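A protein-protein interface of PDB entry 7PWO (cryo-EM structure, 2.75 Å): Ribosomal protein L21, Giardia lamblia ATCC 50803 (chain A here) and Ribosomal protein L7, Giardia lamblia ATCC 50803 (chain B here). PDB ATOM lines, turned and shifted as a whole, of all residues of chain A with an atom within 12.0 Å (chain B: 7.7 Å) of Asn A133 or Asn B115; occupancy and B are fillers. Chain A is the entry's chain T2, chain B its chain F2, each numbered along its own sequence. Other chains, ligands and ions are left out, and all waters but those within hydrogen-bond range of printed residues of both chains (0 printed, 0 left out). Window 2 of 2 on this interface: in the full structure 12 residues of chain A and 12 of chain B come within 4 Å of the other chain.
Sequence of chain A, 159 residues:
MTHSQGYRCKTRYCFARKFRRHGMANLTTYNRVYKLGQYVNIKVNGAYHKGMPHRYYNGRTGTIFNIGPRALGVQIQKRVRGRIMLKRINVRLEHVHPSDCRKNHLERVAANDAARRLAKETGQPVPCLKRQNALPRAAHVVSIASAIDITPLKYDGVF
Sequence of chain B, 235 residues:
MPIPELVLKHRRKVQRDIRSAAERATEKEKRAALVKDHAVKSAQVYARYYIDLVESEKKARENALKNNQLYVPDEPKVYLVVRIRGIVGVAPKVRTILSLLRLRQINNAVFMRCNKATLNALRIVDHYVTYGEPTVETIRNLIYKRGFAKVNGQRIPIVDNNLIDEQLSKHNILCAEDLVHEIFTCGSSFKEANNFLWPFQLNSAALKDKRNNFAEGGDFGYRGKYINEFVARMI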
ATOM      1  N   ASN A 104       3.647  11.282  22.732  1.00  0.00           N
ATOM      2  CA  ASN A 104       4.198  11.339  21.384  1.00  0.00           C
ATOM      3  C   ASN A 104       4.184   9.965  20.725  1.00  0.00           C
ATOM      4  O   ASN A 104       3.893   9.843  19.531  1.00  0.00           O
ATOM      5  CB  ASN A 104       5.614  11.916  21.434  1.00  0.00           C
ATOM      6  CG  ASN A 104       6.258  12.003  20.071  1.00  0.00           C
ATOM      7  OD1 ASN A 104       5.948  12.892  19.278  1.00  0.00           O
ATOM      8  ND2 ASN A 104       7.163  11.072  19.786  1.00  0.00           N
ATOM      9  N   ARG A 108       2.224   8.858  17.294  1.00  0.00           N
ATOM     10  CA  ARG A 108       2.914   8.321  16.126  1.00  0.00           C
ATOM     11  C   ARG A 108       2.364   6.959  15.723  1.00  0.00           C
ATOM     12  O   ARG A 108       2.255   6.666  14.533  1.00  0.00           O
ATOM     13  CB  ARG A 108       4.412   8.227  16.393  1.00  0.00           C
ATOM     14  CG  ARG A 108       5.158   9.544  16.340  1.00  0.00           C
ATOM     15  CD  ARG A 108       6.645   9.267  16.302  1.00  0.00           C
ATOM     16  NE  ARG A 108       7.017   8.571  15.078  1.00  0.00           N
ATOM     17  CZ  ARG A 108       7.571   7.371  15.040  1.00  0.00           C
ATOM     18  NH1 ARG A 108       7.817   6.719  16.161  1.00  0.00           N
ATOM     19  NH2 ARG A 108       7.878   6.822  13.878  1.00  0.00           N
ATOM     20  N   CYS A 128       7.746   6.449   3.797  1.00  0.00           N
ATOM     21  CA  CYS A 128       8.705   6.065   4.822  1.00  0.00           C
ATOM     22  C   CYS A 128       8.227   6.601   6.162  1.00  0.00           C
ATOM     23  O   CYS A 128       7.969   7.801   6.303  1.00  0.00           O
ATOM     24  CB  CYS A 128      10.095   6.598   4.489  1.00  0.00           C
ATOM     25  SG  CYS A 128      11.378   6.136   5.689  1.00  0.00           S
ATOM     26  N   LEU A 129       8.091   5.713   7.144  1.00  0.00           N
ATOM     27  CA  LEU A 129       7.484   6.093   8.406  1.00  0.00           C
ATOM     28  C   LEU A 129       8.490   6.184   9.541  1.00  0.00           C
ATOM     29  O   LEU A 129       8.164   6.754  10.588  1.00  0.00           O
ATOM     30  CB  LEU A 129       6.374   5.101   8.773  1.00  0.00           C
ATOM     31  CG  LEU A 129       5.047   5.432   8.074  1.00  0.00           C
ATOM     32  CD1 LEU A 129       4.065   4.259   8.097  1.00  0.00           C
ATOM     33  CD2 LEU A 129       4.408   6.711   8.561  1.00  0.00           C
ATOM     34  N   LYS A 130       9.702   5.659   9.363  1.00  0.00           N
ATOM     35  CA  LYS A 130      10.721   5.826  10.385  1.00  0.00           C
ATOM     36  C   LYS A 130      11.072   7.295  10.559  1.00  0.00           C
ATOM     37  O   LYS A 130      11.203   8.042   9.587  1.00  0.00           O
ATOM     38  CB  LYS A 130      11.980   5.015  10.065  1.00  0.00           C
ATOM     39  CG  LYS A 130      11.767   3.521  10.127  1.00  0.00           C
ATOM     40  CD  LYS A 130      13.059   2.734   9.981  1.00  0.00           C
ATOM     41  CE  LYS A 130      13.589   2.732   8.569  1.00  0.00           C
ATOM     42  NZ  LYS A 130      14.785   1.855   8.486  1.00  0.00           N
ATOM     43  N   ARG A 131      11.200   7.706  11.817  1.00  0.00           N
ATOM     44  CA  ARG A 131      11.734   9.019  12.137  1.00  0.00           C
ATOM     45  C   ARG A 131      13.131   9.151  11.543  1.00  0.00           C
ATOM     46  O   ARG A 131      13.924   8.207  11.563  1.00  0.00           O
ATOM     47  CB  ARG A 131      11.778   9.191  13.652  1.00  0.00           C
ATOM     48  CG  ARG A 131      10.476   9.622  14.292  1.00  0.00           C
ATOM     49  CD  ARG A 131      10.691   9.859  15.778  1.00  0.00           C
ATOM     50  NE  ARG A 131      10.915   8.570  16.415  1.00  0.00           N
ATOM     51  CZ  ARG A 131      11.128   8.376  17.706  1.00  0.00           C
ATOM     52  NH1 ARG A 131      11.333   7.149  18.150  1.00  0.00           N
ATOM     53  NH2 ARG A 131      11.135   9.395  18.547  1.00  0.00           N
ATOM     54  N   GLN A 132      13.423  10.320  10.990  1.00  0.00           N
ATOM     55  CA  GLN A 132      14.710  10.594  10.361  1.00  0.00           C
ATOM     56  C   GLN A 132      15.294  11.824  11.033  1.00  0.00           C
ATOM     57  O   GLN A 132      14.683  12.896  10.997  1.00  0.00           O
ATOM     58  CB  GLN A 132      14.542  10.803   8.849  1.00  0.00           C
ATOM     59  CG  GLN A 132      15.811  11.040   8.030  1.00  0.00           C
ATOM     60  CD  GLN A 132      16.792   9.892   8.051  1.00  0.00           C
ATOM     61  OE1 GLN A 132      17.819   9.961   8.718  1.00  0.00           O
ATOM     62  NE2 GLN A 132      16.484   8.828   7.320  1.00  0.00           N
ATOM     63  N   ASN A 133      16.454  11.662  11.669  1.00  0.00           N
ATOM     64  CA  ASN A 133      17.114  12.782  12.326  1.00  0.00           C
ATOM     65  C   ASN A 133      17.633  13.753  11.274  1.00  0.00           C
ATOM     66  O   ASN A 133      18.122  13.333  10.225  1.00  0.00           O
ATOM     67  CB  ASN A 133      18.268  12.287  13.197  1.00  0.00           C
ATOM     68  CG  ASN A 133      17.817  11.331  14.286  1.00  0.00           C
ATOM     69  OD1 ASN A 133      16.821  11.559  14.960  1.00  0.00           O
ATOM     70  ND2 ASN A 133      18.553  10.242  14.453  1.00  0.00           N
ATOM     71  N   ALA A 134      17.545  15.052  11.574  1.00  0.00           N
ATOM     72  CA  ALA A 134      17.753  16.127  10.608  1.00  0.00           C
ATOM     73  C   ALA A 134      18.932  15.856   9.691  1.00  0.00           C
ATOM     74  O   ALA A 134      20.061  15.663  10.145  1.00  0.00           O
ATOM     75  CB  ALA A 134      17.966  17.454  11.339  1.00  0.00           C
ATOM     76  N   LEU A 135      18.662  15.835   8.398  1.00  0.00           N
ATOM     77  CA  LEU A 135      19.669  15.598   7.385  1.00  0.00           C
ATOM     78  C   LEU A 135      20.381  16.893   7.018  1.00  0.00           C
ATOM     79  O   LEU A 135      19.918  17.987   7.351  1.00  0.00           O
ATOM     80  CB  LEU A 135      19.018  14.987   6.150  1.00  0.00           C
ATOM     81  CG  LEU A 135      18.362  13.621   6.357  1.00  0.00           C
ATOM     82  CD1 LEU A 135      17.131  13.462   5.488  1.00  0.00           C
ATOM     83  CD2 LEU A 135      19.364  12.525   6.079  1.00  0.00           C
ATOM     84  N   PRO A 136      21.533  16.797   6.356  1.00  0.00           N
ATOM     85  CA  PRO A 136      22.088  17.981   5.698  1.00  0.00           C
ATOM     86  C   PRO A 136      21.136  18.497   4.629  1.00  0.00           C
ATOM     87  O   PRO A 136      20.444  17.730   3.958  1.00  0.00           O
ATOM     88  CB  PRO A 136      23.405  17.477   5.096  1.00  0.00           C
ATOM     89  CG  PRO A 136      23.318  15.997   5.136  1.00  0.00           C
ATOM     90  CD  PRO A 136      22.449  15.648   6.281  1.00  0.00           C
ATOM     91  N   ARG A 137      21.109  19.815   4.482  1.00  0.00           N
ATOM     92  CA  ARG A 137      20.140  20.493   3.637  1.00  0.00           C
ATOM     93  C   ARG A 137      20.551  20.398   2.169  1.00  0.00           C
ATOM     94  O   ARG A 137      21.734  20.314   1.841  1.00  0.00           O
ATOM     95  CB  ARG A 137      20.029  21.943   4.100  1.00  0.00           C
ATOM     96  CG  ARG A 137      21.281  22.705   3.832  1.00  0.00           C
ATOM     97  CD  ARG A 137      21.290  24.101   4.385  1.00  0.00           C
ATOM     98  NE  ARG A 137      21.337  24.030   5.841  1.00  0.00           N
ATOM     99  CZ  ARG A 137      21.217  25.070   6.657  1.00  0.00           C
ATOM    100  NH1 ARG A 137      21.062  26.285   6.166  1.00  0.00           N
ATOM    101  NH2 ARG A 137      21.292  24.896   7.967  1.00  0.00           N
ATOM    102  N   ALA A 138      19.556  20.427   1.285  1.00  0.00           N
ATOM    103  CA  ALA A 138      19.757  20.181  -0.135  1.00  0.00           C
ATOM    104  C   ALA A 138      20.209  21.442  -0.871  1.00  0.00           C
ATOM    105  O   ALA A 138      20.168  22.558  -0.344  1.00  0.00           O
ATOM    106  CB  ALA A 138      18.476  19.650  -0.773  1.00  0.00           C
ATOM    107  N   PRO B  76      27.842  18.146   2.941  1.00  0.00           N
ATOM    108  CA  PRO B  76      28.474  16.825   3.010  1.00  0.00           C
ATOM    109  C   PRO B  76      27.582  15.812   3.704  1.00  0.00           C
ATOM    110  O   PRO B  76      27.029  16.067   4.776  1.00  0.00           O
ATOM    111  CB  PRO B  76      29.757  17.077   3.812  1.00  0.00           C
ATOM    112  CG  PRO B  76      29.909  18.552   3.879  1.00  0.00           C
ATOM    113  CD  PRO B  76      28.553  19.126   3.778  1.00  0.00           C
ATOM    114  N   LYS B  77      27.468  14.640   3.091  1.00  0.00           N
ATOM    115  CA  LYS B  77      26.714  13.546   3.679  1.00  0.00           C
ATOM    116  C   LYS B  77      27.593  12.521   4.380  1.00  0.00           C
ATOM    117  O   LYS B  77      27.118  11.853   5.304  1.00  0.00           O
ATOM    118  CB  LYS B  77      25.874  12.867   2.602  1.00  0.00           C
ATOM    119  CG  LYS B  77      25.194  13.883   1.699  1.00  0.00           C
ATOM    120  CD  LYS B  77      24.041  13.293   0.928  1.00  0.00           C
ATOM    121  CE  LYS B  77      22.837  13.037   1.803  1.00  0.00           C
ATOM    122  NZ  LYS B  77      21.604  12.849   0.987  1.00  0.00           N
ATOM    123  N   MET B 112      31.942   8.044   8.122  1.00  0.00           N
ATOM    124  CA  MET B 112      30.869   8.405   9.039  1.00  0.00           C
ATOM    125  C   MET B 112      29.733   9.080   8.281  1.00  0.00           C
ATOM    126  O   MET B 112      29.967   9.822   7.330  1.00  0.00           O
ATOM    127  CB  MET B 112      31.393   9.333  10.129  1.00  0.00           C
ATOM    128  CG  MET B 112      30.394   9.721  11.188  1.00  0.00           C
ATOM    129  SD  MET B 112      31.217  10.741  12.412  1.00  0.00           S
ATOM    130  CE  MET B 112      29.880  11.179  13.490  1.00  0.00           C
ATOM    131  N   ARG B 113      28.504   8.832   8.721  1.00  0.00           N
ATOM    132  CA  ARG B 113      27.316   9.468   8.165  1.00  0.00           C
ATOM    133  C   ARG B 113      27.051  10.803   8.855  1.00  0.00           C
ATOM    134  O   ARG B 113      27.416  11.001  10.014  1.00  0.00           O
ATOM    135  CB  ARG B 113      26.110   8.540   8.320  1.00  0.00           C
ATOM    136  CG  ARG B 113      24.888   8.928   7.531  1.00  0.00           C
ATOM    137  CD  ARG B 113      23.633   8.285   8.121  1.00  0.00           C
ATOM    138  NE  ARG B 113      23.703   6.826   8.081  1.00  0.00           N
ATOM    139  CZ  ARG B 113      22.969   6.056   7.284  1.00  0.00           C
ATOM    140  NH1 ARG B 113      22.093   6.593   6.454  1.00  0.00           N
ATOM    141  NH2 ARG B 113      23.108   4.742   7.323  1.00  0.00           N
ATOM    142  N   CYS B 114      26.408  11.724   8.142  1.00  0.00           N
ATOM    143  CA  CYS B 114      26.147  13.057   8.672  1.00  0.00           C
ATOM    144  C   CYS B 114      24.653  13.227   8.939  1.00  0.00           C
ATOM    145  O   CYS B 114      23.839  13.123   8.016  1.00  0.00           O
ATOM    146  CB  CYS B 114      26.638  14.129   7.699  1.00  0.00           C
ATOM    147  SG  CYS B 114      28.386  14.538   7.802  1.00  0.00           S
ATOM    148  N   ASN B 115      24.300  13.467  10.200  1.00  0.00           N
ATOM    149  CA  ASN B 115      22.968  13.913  10.604  1.00  0.00           C
ATOM    150  C   ASN B 115      23.123  14.565  11.969  1.00  0.00           C
ATOM    151  O   ASN B 115      24.217  14.598  12.528  1.00  0.00           O
ATOM    152  CB  ASN B 115      21.934  12.773  10.606  1.00  0.00           C
ATOM    153  CG  ASN B 115      22.349  11.584  11.455  1.00  0.00           C
ATOM    154  OD1 ASN B 115      22.654  11.721  12.632  1.00  0.00           O
ATOM    155  ND2 ASN B 115      22.313  10.402  10.870  1.00  0.00           N
ATOM    156  N   LYS B 116      22.024  15.083  12.514  1.00  0.00           N
ATOM    157  CA  LYS B 116      22.148  15.900  13.719  1.00  0.00           C
ATOM    158  C   LYS B 116      22.664  15.089  14.901  1.00  0.00           C
ATOM    159  O   LYS B 116      23.473  15.590  15.692  1.00  0.00           O
ATOM    160  CB  LYS B 116      20.821  16.555  14.060  1.00  0.00           C
ATOM    161  CG  LYS B 116      21.023  17.807  14.879  1.00  0.00           C
ATOM    162  CD  LYS B 116      19.838  18.120  15.747  1.00  0.00           C
ATOM    163  CE  LYS B 116      20.170  19.261  16.680  1.00  0.00           C
ATOM    164  NZ  LYS B 116      19.781  20.572  16.108  1.00  0.00           N
ATOM    165  N   ALA B 117      22.237  13.831  15.018  1.00  0.00           N
ATOM    166  CA  ALA B 117      22.695  12.984  16.115  1.00  0.00           C
ATOM    167  C   ALA B 117      24.205  12.764  16.062  1.00  0.00           C
ATOM    168  O   ALA B 117      24.919  12.996  17.049  1.00  0.00           O
ATOM    169  CB  ALA B 117      21.951  11.652  16.075  1.00  0.00           C
ATOM    170  N   THR B 118      24.713  12.329  14.905  1.00  0.00           N
ATOM    171  CA  THR B 118      26.139  12.058  14.765  1.00  0.00           C
ATOM    172  C   THR B 118      26.967  13.332  14.881  1.00  0.00           C
ATOM    173  O   THR B 118      28.028  13.330  15.517  1.00  0.00           O
ATOM    174  CB  THR B 118      26.420  11.359  13.433  1.00  0.00           C
ATOM    175  OG1 THR B 118      25.676  11.985  12.389  1.00  0.00           O
ATOM    176  CG2 THR B 118      26.048   9.893  13.498  1.00  0.00           C
ATOM    177  N   LEU B 119      26.509  14.431  14.269  1.00  0.00           N
ATOM    178  CA  LEU B 119      27.263  15.681  14.345  1.00  0.00           C
ATOM    179  C   LEU B 119      27.354  16.189  15.775  1.00  0.00           C
ATOM    180  O   LEU B 119      28.413  16.669  16.204  1.00  0.00           O
ATOM    181  CB  LEU B 119      26.649  16.748  13.436  1.00  0.00           C
ATOM    182  CG  LEU B 119      26.512  16.451  11.935  1.00  0.00           C
ATOM    183  CD1 LEU B 119      25.613  17.458  11.233  1.00  0.00           C
ATOM    184  CD2 LEU B 119      27.867  16.356  11.246  1.00  0.00           C
ATOM    185  N   ASN B 120      26.262  16.086  16.534  1.00  0.00           N
ATOM    186  CA  ASN B 120      26.286  16.541  17.913  1.00  0.00           C
ATOM    187  C   ASN B 120      27.070  15.601  18.807  1.00  0.00           C
ATOM    188  O   ASN B 120      27.542  16.026  19.866  1.00  0.00           O
ATOM    189  CB  ASN B 120      24.865  16.699  18.441  1.00  0.00           C
ATOM    190  CG  ASN B 120      24.174  17.917  17.887  1.00  0.00           C
ATOM    191  OD1 ASN B 120      24.675  18.562  16.971  1.00  0.00           O
ATOM    192  ND2 ASN B 120      23.015  18.246  18.443  1.00  0.00           N
ATOM    193  N   ALA B 121      27.207  14.333  18.426  1.00  0.00           N
ATOM    194  CA  ALA B 121      28.119  13.472  19.165  1.00  0.00           C
ATOM    195  C   ALA B 121      29.572  13.838  18.888  1.00  0.00           C
ATOM    196  O   ALA B 121      30.402  13.829  19.803  1.00  0.00           O
ATOM    197  CB  ALA B 121      27.859  12.008  18.831  1.00  0.00           C
ATOM    198  N   LEU B 122      29.893  14.169  17.636  1.00  0.00           N
ATOM    199  CA  LEU B 122      31.281  14.381  17.225  1.00  0.00           C
ATOM    200  C   LEU B 122      31.834  15.723  17.694  1.00  0.00           C
ATOM    201  O   LEU B 122      33.036  15.827  18.008  1.00  0.00           O
ATOM    202  CB  LEU B 122      31.370  14.250  15.706  1.00  0.00           C
ATOM    203  CG  LEU B 122      32.592  14.756  14.950  1.00  0.00           C
ATOM    204  CD1 LEU B 122      33.703  13.742  15.026  1.00  0.00           C
ATOM    205  CD2 LEU B 122      32.201  15.030  13.520  1.00  0.00           C
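Among the printed residues, pairs that only touch across the chains: Asn A133 with Asn B115 (3.9 Å), Ala A134 with Asn B115 (3.4 Å), Pro A136 with Pro B76 (3.7 Å) and Pro A136 with Cys B114 (3.4 Å).
Of the 13 printed residues of chain A, 3 touch a printed residue of chain B.
Printed residues of chain A that touch a printed residue of chain B: Asn A133, Ala A134 and Pro A136.
Of the 13 printed residues of chain B, 4 touch a printed residue of chain A.
Among the printed residues, 5 pairs touch across the chains.
O of Pro B76 sits close to SG of Cys B114 (3.7 Å).
The backbone carbonyl oxygen (O) of Lys B77 sits at hydrogen-bond distance from the backbone NH (N) of Cys B114.
The backbone NH (N) of Ala B117 sits at hydrogen-bond distance from the side-chain amide oxygen (OD1) of Asn B115 (3.2 Å).
OG1 of Thr B118 sits at hydrogen-bond distance from N of Asn B115, 3.0 Å away.
The side-chain amide oxygen of Asn B120 sits close to the backbone carbonyl oxygen of Lys B116 (3.5 Å).
The backbone NH (N) of Lys B116 is in hydrogen-bond range of the backbone carbonyl oxygen (O) of Ala A134, at 3.1 Å.
Of the printed residues of chain B, Ala A134 touches Asn B115 and Lys B116.
Of the printed residues of chain B, Pro A136 touches Pro B76 (3.7 Å) and Cys B114 (3.4 Å).
Lys B77 touches none of the printed residues of chain A.
No residue of chain A comes within 4 Å of Arg B113.
Of chain A, only Pro A136 comes within 4 Å of Cys B114.
Asn B115 touches just these residues of chain A: Asn A133 (3.9 Å) and Ala A134 (3.4 Å).
No residue of chain A comes within 4 Å of Ala B117.
No residue of chain A comes within 4 Å of Thr B118.
The nearest residue of chain A that does not touch Asn B115 is Pro A136 (4.7 Å).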
